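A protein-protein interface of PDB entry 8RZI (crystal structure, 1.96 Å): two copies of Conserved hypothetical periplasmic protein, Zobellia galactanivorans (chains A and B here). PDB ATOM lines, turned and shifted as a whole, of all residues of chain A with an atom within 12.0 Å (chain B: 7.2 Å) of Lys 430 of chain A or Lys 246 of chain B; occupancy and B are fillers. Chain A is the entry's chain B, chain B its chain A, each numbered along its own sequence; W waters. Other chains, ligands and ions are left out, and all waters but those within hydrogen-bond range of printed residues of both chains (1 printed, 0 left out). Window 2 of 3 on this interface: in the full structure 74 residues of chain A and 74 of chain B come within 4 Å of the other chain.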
ATOM      1  N   PHE A 418      -8.249 -11.839  -2.708  1.00  0.00           N
ATOM      2  CA  PHE A 418      -8.904 -10.553  -2.945  1.00  0.00           C
ATOM      3  C   PHE A 418      -7.880  -9.423  -2.940  1.00  0.00           C
ATOM      4  O   PHE A 418      -6.993  -9.372  -2.083  1.00  0.00           O
ATOM      5  CB  PHE A 418      -9.987 -10.272  -1.878  1.00  0.00           C
ATOM      6  CG  PHE A 418     -10.657  -8.934  -2.034  1.00  0.00           C
ATOM      7  CD1 PHE A 418     -10.145  -7.805  -1.423  1.00  0.00           C
ATOM      8  CD2 PHE A 418     -11.778  -8.800  -2.828  1.00  0.00           C
ATOM      9  CE1 PHE A 418     -10.752  -6.567  -1.589  1.00  0.00           C
ATOM     10  CE2 PHE A 418     -12.400  -7.562  -3.000  1.00  0.00           C
ATOM     11  CZ  PHE A 418     -11.878  -6.441  -2.377  1.00  0.00           C
ATOM     12  N   THR A 420      -7.828  -4.990  -4.135  1.00  0.00           N
ATOM     13  CA  THR A 420      -8.389  -3.858  -4.853  1.00  0.00           C
ATOM     14  C   THR A 420      -7.508  -3.428  -6.029  1.00  0.00           C
ATOM     15  O   THR A 420      -7.910  -2.542  -6.784  1.00  0.00           O
ATOM     16  CB  THR A 420      -8.612  -2.693  -3.885  1.00  0.00           C
ATOM     17  OG1 THR A 420      -7.372  -2.356  -3.263  1.00  0.00           O
ATOM     18  CG2 THR A 420      -9.621  -3.091  -2.785  1.00  0.00           C
ATOM     19  N   ASP A 421      -6.334  -4.051  -6.216  1.00  0.00           N
ATOM     20  CA  ASP A 421      -5.431  -3.652  -7.303  1.00  0.00           C
ATOM     21  C   ASP A 421      -6.037  -3.908  -8.672  1.00  0.00           C
ATOM     22  O   ASP A 421      -5.672  -3.237  -9.646  1.00  0.00           O
ATOM     23  CB  ASP A 421      -4.102  -4.402  -7.206  1.00  0.00           C
ATOM     24  CG  ASP A 421      -3.224  -3.891  -6.095  1.00  0.00           C
ATOM     25  OD1 ASP A 421      -3.538  -2.813  -5.531  1.00  0.00           O
ATOM     26  OD2 ASP A 421      -2.218  -4.577  -5.784  1.00  0.00           O
ATOM     27  N   LEU A 422      -6.937  -4.879  -8.777  1.00  0.00           N
ATOM     28  CA  LEU A 422      -7.555  -5.204 -10.053  1.00  0.00           C
ATOM     29  C   LEU A 422      -8.847  -4.432 -10.296  1.00  0.00           C
ATOM     30  O   LEU A 422      -9.507  -4.655 -11.319  1.00  0.00           O
ATOM     31  CB  LEU A 422      -7.811  -6.713 -10.137  1.00  0.00           C
ATOM     32  CG  LEU A 422      -6.527  -7.529 -10.368  1.00  0.00           C
ATOM     33  CD1 LEU A 422      -6.786  -9.029 -10.252  1.00  0.00           C
ATOM     34  CD2 LEU A 422      -5.939  -7.204 -11.720  1.00  0.00           C
ATOM     35  N   MET A 423      -9.230  -3.544  -9.384  1.00  0.00           N
ATOM     36  CA  MET A 423     -10.491  -2.833  -9.517  1.00  0.00           C
ATOM     37  C   MET A 423     -10.265  -1.511 -10.245  1.00  0.00           C
ATOM     38  O   MET A 423      -9.134  -1.140 -10.580  1.00  0.00           O
ATOM     39  CB  MET A 423     -11.135  -2.619  -8.138  1.00  0.00           C
ATOM     40  CG  MET A 423     -11.539  -3.922  -7.464  1.00  0.00           C
ATOM     41  SD  MET A 423     -12.218  -3.763  -5.793  1.00  0.00           S
ATOM     42  CE  MET A 423     -13.672  -2.774  -6.169  1.00  0.00           C
ATOM     43  N   GLN A 424     -11.365  -0.824 -10.537  1.00  0.00           N
ATOM     44  CA  GLN A 424     -11.312   0.451 -11.237  1.00  0.00           C
ATOM     45  C   GLN A 424     -11.638   1.580 -10.274  1.00  0.00           C
ATOM     46  O   GLN A 424     -12.428   1.409  -9.346  1.00  0.00           O
ATOM     47  CB  GLN A 424     -12.284   0.485 -12.409  1.00  0.00           C
ATOM     48  CG  GLN A 424     -12.100   1.705 -13.304  1.00  0.00           C
ATOM     49  CD  GLN A 424     -13.125   1.777 -14.410  1.00  0.00           C
ATOM     50  OE1 GLN A 424     -13.944   0.874 -14.571  1.00  0.00           O
ATOM     51  NE2 GLN A 424     -13.091   2.853 -15.177  1.00  0.00           N
ATOM     52  N   ARG A 425     -11.010   2.727 -10.482  1.00  0.00           N
ATOM     53  CA  ARG A 425     -11.261   3.912  -9.681  1.00  0.00           C
ATOM     54  C   ARG A 425     -11.821   5.019 -10.565  1.00  0.00           C
ATOM     55  O   ARG A 425     -11.496   5.117 -11.754  1.00  0.00           O
ATOM     56  CB  ARG A 425     -10.008   4.383  -8.976  1.00  0.00           C
ATOM     57  CG  ARG A 425      -9.574   3.435  -7.881  1.00  0.00           C
ATOM     58  CD  ARG A 425      -8.188   3.736  -7.341  1.00  0.00           C
ATOM     59  NE  ARG A 425      -7.785   2.739  -6.349  1.00  0.00           N
ATOM     60  CZ  ARG A 425      -8.127   2.791  -5.059  1.00  0.00           C
ATOM     61  NH1 ARG A 425      -8.869   3.796  -4.600  1.00  0.00           N
ATOM     62  NH2 ARG A 425      -7.734   1.839  -4.224  1.00  0.00           N
ATOM     63  N   ASP A 426     -12.683   5.850  -9.972  1.00  0.00           N
ATOM     64  CA  ASP A 426     -13.380   6.892 -10.709  1.00  0.00           C
ATOM     65  C   ASP A 426     -12.570   8.190 -10.659  1.00  0.00           C
ATOM     66  O   ASP A 426     -11.455   8.244 -10.133  1.00  0.00           O
ATOM     67  CB  ASP A 426     -14.807   7.064 -10.167  1.00  0.00           C
ATOM     68  CG  ASP A 426     -14.845   7.610  -8.740  1.00  0.00           C
ATOM     69  OD1 ASP A 426     -13.815   8.043  -8.174  1.00  0.00           O
ATOM     70  OD2 ASP A 426     -15.950   7.605  -8.164  1.00  0.00           O
ATOM     71  N   ALA A 427     -13.149   9.266 -11.188  1.00  0.00           N
ATOM     72  CA  ALA A 427     -12.403  10.503 -11.359  1.00  0.00           C
ATOM     73  C   ALA A 427     -11.953  11.078 -10.028  1.00  0.00           C
ATOM     74  O   ALA A 427     -11.029  11.901  -9.999  1.00  0.00           O
ATOM     75  CB  ALA A 427     -13.251  11.511 -12.139  1.00  0.00           C
ATOM     76  N   GLU A 428     -12.569  10.644  -8.924  1.00  0.00           N
ATOM     77  CA  GLU A 428     -12.191  11.109  -7.597  1.00  0.00           C
ATOM     78  C   GLU A 428     -11.248  10.139  -6.905  1.00  0.00           C
ATOM     79  O   GLU A 428     -10.909  10.348  -5.733  1.00  0.00           O
ATOM     80  CB  GLU A 428     -13.444  11.338  -6.735  1.00  0.00           C
ATOM     81  CG  GLU A 428     -14.328  12.509  -7.207  1.00  0.00           C
ATOM     82  N   GLY A 429     -10.803   9.099  -7.610  1.00  0.00           N
ATOM     83  CA  GLY A 429      -9.941   8.098  -7.022  1.00  0.00           C
ATOM     84  C   GLY A 429     -10.638   7.051  -6.176  1.00  0.00           C
ATOM     85  O   GLY A 429      -9.948   6.265  -5.514  1.00  0.00           O
ATOM     86  N   LYS A 430     -11.976   7.008  -6.170  1.00  0.00           N
ATOM     87  CA  LYS A 430     -12.712   6.059  -5.330  1.00  0.00           C
ATOM     88  C   LYS A 430     -12.944   4.763  -6.085  1.00  0.00           C
ATOM     89  O   LYS A 430     -13.226   4.782  -7.283  1.00  0.00           O
ATOM     90  CB  LYS A 430     -14.065   6.614  -4.904  1.00  0.00           C
ATOM     91  CG  LYS A 430     -14.010   7.868  -4.076  1.00  0.00           C
ATOM     92  CD  LYS A 430     -15.436   8.348  -3.799  1.00  0.00           C
ATOM     93  CE  LYS A 430     -15.439   9.776  -3.275  1.00  0.00           C
ATOM     94  NZ  LYS A 430     -16.793  10.205  -2.825  1.00  0.00           N
ATOM     95  N   LEU A 431     -12.866   3.641  -5.368  1.00  0.00           N
ATOM     96  CA  LEU A 431     -13.129   2.353  -6.001  1.00  0.00           C
ATOM     97  C   LEU A 431     -14.531   2.332  -6.596  1.00  0.00           C
ATOM     98  O   LEU A 431     -15.474   2.919  -6.047  1.00  0.00           O
ATOM     99  CB  LEU A 431     -12.976   1.206  -5.001  1.00  0.00           C
ATOM    100  CG  LEU A 431     -11.556   0.899  -4.526  1.00  0.00           C
ATOM    101  CD1 LEU A 431     -11.616  -0.064  -3.334  1.00  0.00           C
ATOM    102  CD2 LEU A 431     -10.769   0.297  -5.665  1.00  0.00           C
ATOM    103  N   MET A 432     -14.659   1.666  -7.737  1.00  0.00           N
ATOM    104  CA  MET A 432     -15.940   1.537  -8.407  1.00  0.00           C
ATOM    105  C   MET A 432     -16.476   0.125  -8.218  1.00  0.00           C
ATOM    106  O   MET A 432     -15.713  -0.841  -8.116  1.00  0.00           O
ATOM    107  CB  MET A 432     -15.834   1.875  -9.901  1.00  0.00           C
ATOM    108  CG  MET A 432     -15.471   3.343 -10.181  1.00  0.00           C
ATOM    109  SD  MET A 432     -14.908   3.585 -11.893  1.00  0.00           S
ATOM    110  CE  MET A 432     -16.267   2.861 -12.817  1.00  0.00           C
ATOM    111  N   ASN A 433     -17.804   0.030  -8.146  1.00  0.00           N
ATOM    112  CA  ASN A 433     -18.515  -1.231  -7.966  1.00  0.00           C
ATOM    113  C   ASN A 433     -18.144  -1.904  -6.652  1.00  0.00           C
ATOM    114  O   ASN A 433     -18.128  -3.133  -6.555  1.00  0.00           O
ATOM    115  CB  ASN A 433     -18.282  -2.167  -9.161  1.00  0.00           C
ATOM    116  CG  ASN A 433     -19.236  -1.851 -10.313  1.00  0.00           C
ATOM    117  OD1 ASN A 433     -20.058  -0.946 -10.191  1.00  0.00           O
ATOM    118  ND2 ASN A 433     -19.147  -2.598 -11.411  1.00  0.00           N
ATOM    119  N   THR A 434     -17.842  -1.112  -5.622  1.00  0.00           N
ATOM    120  CA  THR A 434     -17.696  -1.694  -4.290  1.00  0.00           C
ATOM    121  C   THR A 434     -18.950  -2.448  -3.854  1.00  0.00           C
ATOM    122  O   THR A 434     -18.850  -3.389  -3.056  1.00  0.00           O
ATOM    123  CB  THR A 434     -17.358  -0.620  -3.263  1.00  0.00           C
ATOM    124  OG1 THR A 434     -18.325   0.425  -3.348  1.00  0.00           O
ATOM    125  CG2 THR A 434     -15.964  -0.052  -3.534  1.00  0.00           C
ATOM    126  N   GLY A 435     -20.115  -2.098  -4.391  1.00  0.00           N
ATOM    127  CA  GLY A 435     -21.327  -2.800  -4.030  1.00  0.00           C
ATOM    128  C   GLY A 435     -21.731  -3.850  -5.043  1.00  0.00           C
ATOM    129  O   GLY A 435     -22.877  -4.310  -5.026  1.00  0.00           O
ATOM    130  N   SER A 436     -20.810  -4.253  -5.946  1.00  0.00           N
ATOM    131  CA  SER A 436     -21.210  -5.144  -7.025  1.00  0.00           C
ATOM    132  C   SER A 436     -20.111  -6.187  -7.283  1.00  0.00           C
ATOM    133  O   SER A 436     -19.349  -6.102  -8.261  1.00  0.00           O
ATOM    134  CB  SER A 436     -21.542  -4.330  -8.269  1.00  0.00           C
ATOM    135  OG  SER A 436     -22.180  -5.170  -9.205  1.00  0.00           O
ATOM    136  N   ALA A 439     -18.695  -7.825 -10.671  1.00  0.00           N
ATOM    137  CA  ALA A 439     -18.196  -6.964 -11.746  1.00  0.00           C
ATOM    138  C   ALA A 439     -17.281  -5.884 -11.154  1.00  0.00           C
ATOM    139  O   ALA A 439     -17.539  -4.688 -11.231  1.00  0.00           O
ATOM    140  CB  ALA A 439     -19.369  -6.363 -12.534  1.00  0.00           C
ATOM    141  N   ARG A 440     -16.203  -6.317 -10.502  1.00  0.00           N
ATOM    142  CA  ARG A 440     -15.248  -5.400  -9.889  1.00  0.00           C
ATOM    143  C   ARG A 440     -13.934  -5.289 -10.655  1.00  0.00           C
ATOM    144  O   ARG A 440     -13.251  -4.263 -10.543  1.00  0.00           O
ATOM    145  CB  ARG A 440     -14.950  -5.837  -8.445  1.00  0.00           C
ATOM    146  CG  ARG A 440     -16.084  -5.486  -7.450  1.00  0.00           C
ATOM    147  CD  ARG A 440     -15.787  -6.018  -6.061  1.00  0.00           C
ATOM    148  NE  ARG A 440     -16.825  -5.641  -5.097  1.00  0.00           N
ATOM    149  CZ  ARG A 440     -17.120  -6.343  -4.009  1.00  0.00           C
ATOM    150  NH1 ARG A 440     -18.087  -5.943  -3.180  1.00  0.00           N
ATOM    151  NH2 ARG A 440     -16.465  -7.471  -3.770  1.00  0.00           N
ATOM    152  N   VAL A 441     -13.542  -6.319 -11.400  1.00  0.00           N
ATOM    153  CA  VAL A 441     -12.283  -6.246 -12.133  1.00  0.00           C
ATOM    154  C   VAL A 441     -12.457  -5.313 -13.318  1.00  0.00           C
ATOM    155  O   VAL A 441     -13.381  -5.483 -14.122  1.00  0.00           O
ATOM    156  CB  VAL A 441     -11.833  -7.642 -12.590  1.00  0.00           C
ATOM    157  CG1 VAL A 441     -10.540  -7.544 -13.431  1.00  0.00           C
ATOM    158  CG2 VAL A 441     -11.615  -8.532 -11.385  1.00  0.00           C
ATOM    159  N   ASP A 442     -11.570  -4.331 -13.434  1.00  0.00           N
ATOM    160  CA  ASP A 442     -11.575  -3.455 -14.599  1.00  0.00           C
ATOM    161  C   ASP A 442     -11.494  -4.304 -15.871  1.00  0.00           C
ATOM    162  O   ASP A 442     -10.632  -5.194 -15.962  1.00  0.00           O
ATOM    163  CB  ASP A 442     -10.386  -2.486 -14.536  1.00  0.00           C
ATOM    164  CG  ASP A 442     -10.453  -1.384 -15.608  1.00  0.00           C
ATOM    165  OD1 ASP A 442     -10.876  -1.662 -16.753  1.00  0.00           O
ATOM    166  OD2 ASP A 442     -10.063  -0.236 -15.303  1.00  0.00           O
ATOM    167  N   LYS A 444     -10.163  -3.780 -18.551  1.00  0.00           N
ATOM    168  CA  LYS A 444      -8.857  -3.707 -19.189  1.00  0.00           C
ATOM    169  C   LYS A 444      -7.897  -4.759 -18.657  1.00  0.00           C
ATOM    170  O   LYS A 444      -6.843  -4.973 -19.271  1.00  0.00           O
ATOM    171  CB  LYS A 444      -8.255  -2.308 -19.013  1.00  0.00           C
ATOM    172  CG  LYS A 444      -7.735  -2.006 -17.629  1.00  0.00           C
ATOM    173  CD  LYS A 444      -7.181  -0.588 -17.622  1.00  0.00           C
ATOM    174  CE  LYS A 444      -6.739  -0.116 -16.254  1.00  0.00           C
ATOM    175  NZ  LYS A 444      -6.608   1.385 -16.208  1.00  0.00           N
ATOM    176  N   PHE A 445      -8.229  -5.405 -17.528  1.00  0.00           N
ATOM    177  CA  PHE A 445      -7.434  -6.494 -16.989  1.00  0.00           C
ATOM    178  C   PHE A 445      -7.955  -7.864 -17.383  1.00  0.00           C
ATOM    179  O   PHE A 445      -7.271  -8.858 -17.115  1.00  0.00           O
ATOM    180  CB  PHE A 445      -7.406  -6.452 -15.456  1.00  0.00           C
ATOM    181  CG  PHE A 445      -6.900  -5.164 -14.877  1.00  0.00           C
ATOM    182  CD1 PHE A 445      -5.799  -4.527 -15.407  1.00  0.00           C
ATOM    183  CD2 PHE A 445      -7.535  -4.604 -13.782  1.00  0.00           C
ATOM    184  CE1 PHE A 445      -5.338  -3.329 -14.857  1.00  0.00           C
ATOM    185  CE2 PHE A 445      -7.095  -3.426 -13.229  1.00  0.00           C
ATOM    186  CZ  PHE A 445      -5.986  -2.783 -13.769  1.00  0.00           C
ATOM    187  N   ASN A 478     -18.391   2.718 -20.029  1.00  0.00           N
ATOM    188  CA  ASN A 478     -17.197   2.581 -19.207  1.00  0.00           C
ATOM    189  C   ASN A 478     -16.704   1.139 -19.242  1.00  0.00           C
ATOM    190  O   ASN A 478     -17.439   0.207 -18.890  1.00  0.00           O
ATOM    191  CB  ASN A 478     -17.492   3.016 -17.774  1.00  0.00           C
ATOM    192  CG  ASN A 478     -16.320   2.759 -16.830  1.00  0.00           C
ATOM    193  OD1 ASN A 478     -15.509   3.646 -16.579  1.00  0.00           O
ATOM    194  ND2 ASN A 478     -16.240   1.548 -16.296  1.00  0.00           N
ATOM    195  N   GLU B  54     -19.046  -1.063  15.087  1.00  0.00           N
ATOM    196  CA  GLU B  54     -18.553   0.261  15.465  1.00  0.00           C
ATOM    197  C   GLU B  54     -18.635   0.514  16.965  1.00  0.00           C
ATOM    198  O   GLU B  54     -18.407   1.649  17.406  1.00  0.00           O
ATOM    199  CB  GLU B  54     -19.327   1.354  14.715  1.00  0.00           C
ATOM    200  CG  GLU B  54     -18.957   1.443  13.237  1.00  0.00           C
ATOM    201  CD  GLU B  54     -19.931   2.287  12.408  1.00  0.00           C
ATOM    202  OE1 GLU B  54     -20.951   2.766  12.981  1.00  0.00           O
ATOM    203  OE2 GLU B  54     -19.674   2.465  11.178  1.00  0.00           O
ATOM    204  N   TYR B 241     -22.877  -1.264   2.356  1.00  0.00           N
ATOM    205  CA  TYR B 241     -23.730  -0.120   2.044  1.00  0.00           C
ATOM    206  C   TYR B 241     -23.321   1.147   2.790  1.00  0.00           C
ATOM    207  O   TYR B 241     -23.662   2.250   2.353  1.00  0.00           O
ATOM    208  CB  TYR B 241     -25.197  -0.449   2.348  1.00  0.00           C
ATOM    209  CG  TYR B 241     -25.480  -0.963   3.751  1.00  0.00           C
ATOM    210  CD1 TYR B 241     -25.363  -2.320   4.052  1.00  0.00           C
ATOM    211  CD2 TYR B 241     -25.912  -0.100   4.765  1.00  0.00           C
ATOM    212  CE1 TYR B 241     -25.649  -2.799   5.320  1.00  0.00           C
ATOM    213  CE2 TYR B 241     -26.204  -0.576   6.052  1.00  0.00           C
ATOM    214  CZ  TYR B 241     -26.069  -1.925   6.312  1.00  0.00           C
ATOM    215  OH  TYR B 241     -26.334  -2.416   7.567  1.00  0.00           O
ATOM    216  N   LEU B 242     -22.609   1.022   3.905  1.00  0.00           N
ATOM    217  CA  LEU B 242     -22.153   2.206   4.621  1.00  0.00           C
ATOM    218  C   LEU B 242     -20.974   2.858   3.914  1.00  0.00           C
ATOM    219  O   LEU B 242     -20.641   4.010   4.205  1.00  0.00           O
ATOM    220  CB  LEU B 242     -21.767   1.838   6.062  1.00  0.00           C
ATOM    221  CG  LEU B 242     -22.869   1.161   6.884  1.00  0.00           C
ATOM    222  CD1 LEU B 242     -22.334   0.517   8.178  1.00  0.00           C
ATOM    223  CD2 LEU B 242     -23.959   2.158   7.202  1.00  0.00           C
ATOM    224  N   PHE B 243     -20.340   2.158   2.982  1.00  0.00           N
ATOM    225  CA  PHE B 243     -19.083   2.617   2.424  1.00  0.00           C
ATOM    226  C   PHE B 243     -19.108   2.828   0.920  1.00  0.00           C
ATOM    227  O   PHE B 243     -18.096   3.282   0.366  1.00  0.00           O
ATOM    228  CB  PHE B 243     -17.967   1.623   2.760  1.00  0.00           C
ATOM    229  CG  PHE B 243     -17.764   1.430   4.221  1.00  0.00           C
ATOM    230  CD1 PHE B 243     -16.975   2.307   4.931  1.00  0.00           C
ATOM    231  CD2 PHE B 243     -18.358   0.372   4.885  1.00  0.00           C
ATOM    232  CE1 PHE B 243     -16.777   2.138   6.289  1.00  0.00           C
ATOM    233  CE2 PHE B 243     -18.171   0.189   6.247  1.00  0.00           C
ATOM    234  CZ  PHE B 243     -17.380   1.072   6.954  1.00  0.00           C
ATOM    235  N   ASN B 244     -20.214   2.518   0.241  1.00  0.00           N
ATOM    236  CA  ASN B 244     -20.207   2.607  -1.212  1.00  0.00           C
ATOM    237  C   ASN B 244     -19.990   4.040  -1.668  1.00  0.00           C
ATOM    238  O   ASN B 244     -19.271   4.284  -2.642  1.00  0.00           O
ATOM    239  CB  ASN B 244     -21.504   2.042  -1.781  1.00  0.00           C
ATOM    240  CG  ASN B 244     -21.548   0.519  -1.716  1.00  0.00           C
ATOM    241  OD1 ASN B 244     -20.507  -0.157  -1.744  1.00  0.00           O
ATOM    242  ND2 ASN B 244     -22.753  -0.027  -1.627  1.00  0.00           N
ATOM    243  N   ALA B 245     -20.578   5.004  -0.961  1.00  0.00           N
ATOM    244  CA  ALA B 245     -20.406   6.396  -1.356  1.00  0.00           C
ATOM    245  C   ALA B 245     -18.968   6.860  -1.132  1.00  0.00           C
ATOM    246  O   ALA B 245     -18.469   7.712  -1.878  1.00  0.00           O
ATOM    247  CB  ALA B 245     -21.398   7.288  -0.600  1.00  0.00           C
ATOM    248  N   LYS B 246     -18.288   6.305  -0.123  1.00  0.00           N
ATOM    249  CA  LYS B 246     -16.869   6.583   0.063  1.00  0.00           C
ATOM    250  C   LYS B 246     -16.000   5.812  -0.929  1.00  0.00           C
ATOM    251  O   LYS B 246     -14.810   6.117  -1.062  1.00  0.00           O
ATOM    252  CB  LYS B 246     -16.424   6.227   1.487  1.00  0.00           C
ATOM    253  CG  LYS B 246     -17.040   7.049   2.628  1.00  0.00           C
ATOM    254  CD  LYS B 246     -16.729   6.380   3.985  1.00  0.00           C
ATOM    255  CE  LYS B 246     -17.260   7.185   5.170  1.00  0.00           C
ATOM    256  NZ  LYS B 246     -17.607   6.303   6.338  1.00  0.00           N
ATOM    257  N   GLY B 247     -16.552   4.809  -1.605  1.00  0.00           N
ATOM    258  CA  GLY B 247     -15.747   4.048  -2.547  1.00  0.00           C
ATOM    259  C   GLY B 247     -14.608   3.294  -1.893  1.00  0.00           C
ATOM    260  O   GLY B 247     -13.489   3.309  -2.410  1.00  0.00           O
ATOM    261  N   VAL B 248     -14.866   2.652  -0.752  1.00  0.00           N
ATOM    262  CA  VAL B 248     -13.910   1.762  -0.112  1.00  0.00           C
ATOM    263  C   VAL B 248     -14.627   0.475   0.291  1.00  0.00           C
ATOM    264  O   VAL B 248     -15.852   0.398   0.333  1.00  0.00           O
ATOM    265  CB  VAL B 248     -13.242   2.405   1.119  1.00  0.00           C
ATOM    266  CG1 VAL B 248     -12.622   3.763   0.775  1.00  0.00           C
ATOM    267  CG2 VAL B 248     -14.233   2.517   2.239  1.00  0.00           C
ATOM    268  N   MET B 249     -13.835  -0.538   0.610  1.00  0.00           N
ATOM    269  CA  MET B 249     -14.368  -1.847   0.985  1.00  0.00           C
ATOM    270  C   MET B 249     -14.741  -1.860   2.468  1.00  0.00           C
ATOM    271  O   MET B 249     -14.051  -1.259   3.293  1.00  0.00           O
ATOM    272  CB  MET B 249     -13.323  -2.930   0.697  1.00  0.00           C
ATOM    273  CG  MET B 249     -12.903  -3.037  -0.792  1.00  0.00           C
ATOM    274  SD  MET B 249     -14.329  -3.157  -1.930  1.00  0.00           S
ATOM    275  CE  MET B 249     -15.129  -4.672  -1.377  1.00  0.00           C
ATOM    276  N   TYR B 252     -16.006  -4.708   7.972  1.00  0.00           N
ATOM    277  CA  TYR B 252     -16.827  -5.373   8.975  1.00  0.00           C
ATOM    278  C   TYR B 252     -17.168  -6.798   8.552  1.00  0.00           C
ATOM    279  O   TYR B 252     -17.009  -7.182   7.390  1.00  0.00           O
ATOM    280  CB  TYR B 252     -18.111  -4.592   9.196  1.00  0.00           C
ATOM    281  CG  TYR B 252     -17.904  -3.146   9.561  1.00  0.00           C
ATOM    282  CD1 TYR B 252     -16.809  -2.740  10.335  1.00  0.00           C
ATOM    283  CD2 TYR B 252     -18.811  -2.183   9.154  1.00  0.00           C
ATOM    284  CE1 TYR B 252     -16.637  -1.397  10.673  1.00  0.00           C
ATOM    285  CE2 TYR B 252     -18.642  -0.850   9.483  1.00  0.00           C
ATOM    286  CZ  TYR B 252     -17.568  -0.463  10.241  1.00  0.00           C
ATOM    287  OH  TYR B 252     -17.432   0.873  10.545  1.00  0.00           O
HETATM  288  O   HOH W   1     -11.040   4.243  -2.282  1.00  0.00           O
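OD1 of Asn 244 of chain B is in hydrogen-bond range of OG1 of Thr 434 of chain A.
OD1 of Asn 244 of chain B is in hydrogen-bond range of N of Gly 435 of chain A (3.3 Å).
The backbone carbonyl oxygen of Ala 245 of chain B lies within hydrogen-bond range of the side-chain amino group of Lys 430 of chain A (3.1 Å).
The backbone NH (N) of Leu 431 of chain A lies within hydrogen-bond range of the backbone carbonyl oxygen (O) of Gly 247 of chain B, at 3.0 Å.
The backbone carbonyl oxygen (O) of Phe 243 of chain B is in hydrogen-bond range of the backbone NH (N) of Val 248 of chain B (3.5 Å).
The backbone NH (N) of Lys 430 of chain A lies within hydrogen-bond range of the side-chain carboxylate (OD1) of Asp 426 of chain A, at 2.9 Å.
O of Asn 433 of chain A is in hydrogen-bond range of NE of Arg 440 of chain A, 3.2 Å away.
NH1 of Arg 440 of chain A sits at hydrogen-bond distance from O of Thr 434 of chain A (2.7 Å).
CZ of Phe 418 of chain A touches CE of Met 249 of chain B, at 3.8 Å.
CG of Met 249 of chain B touches CG2 of Thr 420 of chain A (3.8 Å).
Lys 430 of chain A touches Lys 246 of chain B (CG to O, 3.6 Å).
Lys 430 of chain A touches Gly 247 of chain B.
Thr 434 of chain A touches Gly 247 of chain B (CG2 to C, 3.97 Å).
Thr 434 of chain A touches Val 248 of chain B (CG2 to O, 3.9 Å).
Thr 434 of chain A touches Met 249 of chain B (CG2 to SD, 3.9 Å).
Arg 440 of chain A touches Met 249 of chain B (NH1 to CE, 3.7 Å).
Lys 430 of chain A touches three residues of chain B.
No residue of chain A comes within 4 Å of Leu 242 of chain B.
No residue of chain A comes within 4 Å of Phe 243 of chain B.
Asn 244 of chain B touches just these residues of chain A: Thr 434 and Gly 435.
Of chain A, only Lys 430 (3.1 Å) comes within 4 Å of Ala 245 of chain B.
Of chain A, only Lys 430 (3.9 Å), Leu 431 (3.0 Å) and Thr 434 (3.97 Å) come within 4 Å of Gly 247 of chain B.
Val 248 of chain B touches just one residue of chain A: Thr 434 (3.9 Å).
Printed residues of chain B within 4 Å of Leu 431 of chain A: Gly 247 (3.0 Å).
Of the printed residues of chain B, Arg 440 of chain A touches Met 249.
Of the printed residues of chain B, Thr 434 of chain A touches Asn 244, Gly 247, Val 248 and Met 249.
Of the printed residues of chain A, Met 249 of chain B touches Phe 418, Thr 420, Thr 434 and Arg 440.
Of the printed residues of chain B, Thr 420 of chain A touches Met 249.
Lys 444 of chain A touches none of the printed residues of chain B.
Met 423 of chain A touches none of the printed residues of chain B.
The nearest residue of chain B that does not touch Lys 430 of chain A is Asn 244 of chain B (5.7 Å).
The nearest residue of chain A that does not touch Lys 246 of chain B is Leu 431 of chain A (5.3 Å).
The nearest printed residue of chain B that does not touch Thr 434 of chain A is Phe 243 of chain B (4.7 Å).
Hydrophobic or aromatic side chains of chain A within 4 Å of the printed part of chain B: Phe 418 and Leu 431.
Along chain A the printed residues that touch a printed residue of chain B span positions 418 to 440.
Among the printed residues, 12 pairs touch across the chains.
Among the printed residues, no Asp or Glu carboxylate lies within 4 Å of a Lys or Arg side-chain nitrogen of the other chain.
No position is printed for both chains.
Of the 12 pairs that touch across the chains among the printed residues, none has its exchanged pair printed and touching as well.
Water W1 lies within hydrogen-bond range of O of Gly 247 of chain B (2.6 Å) and NH1 of Arg 425 of chain A (3.2 Å).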
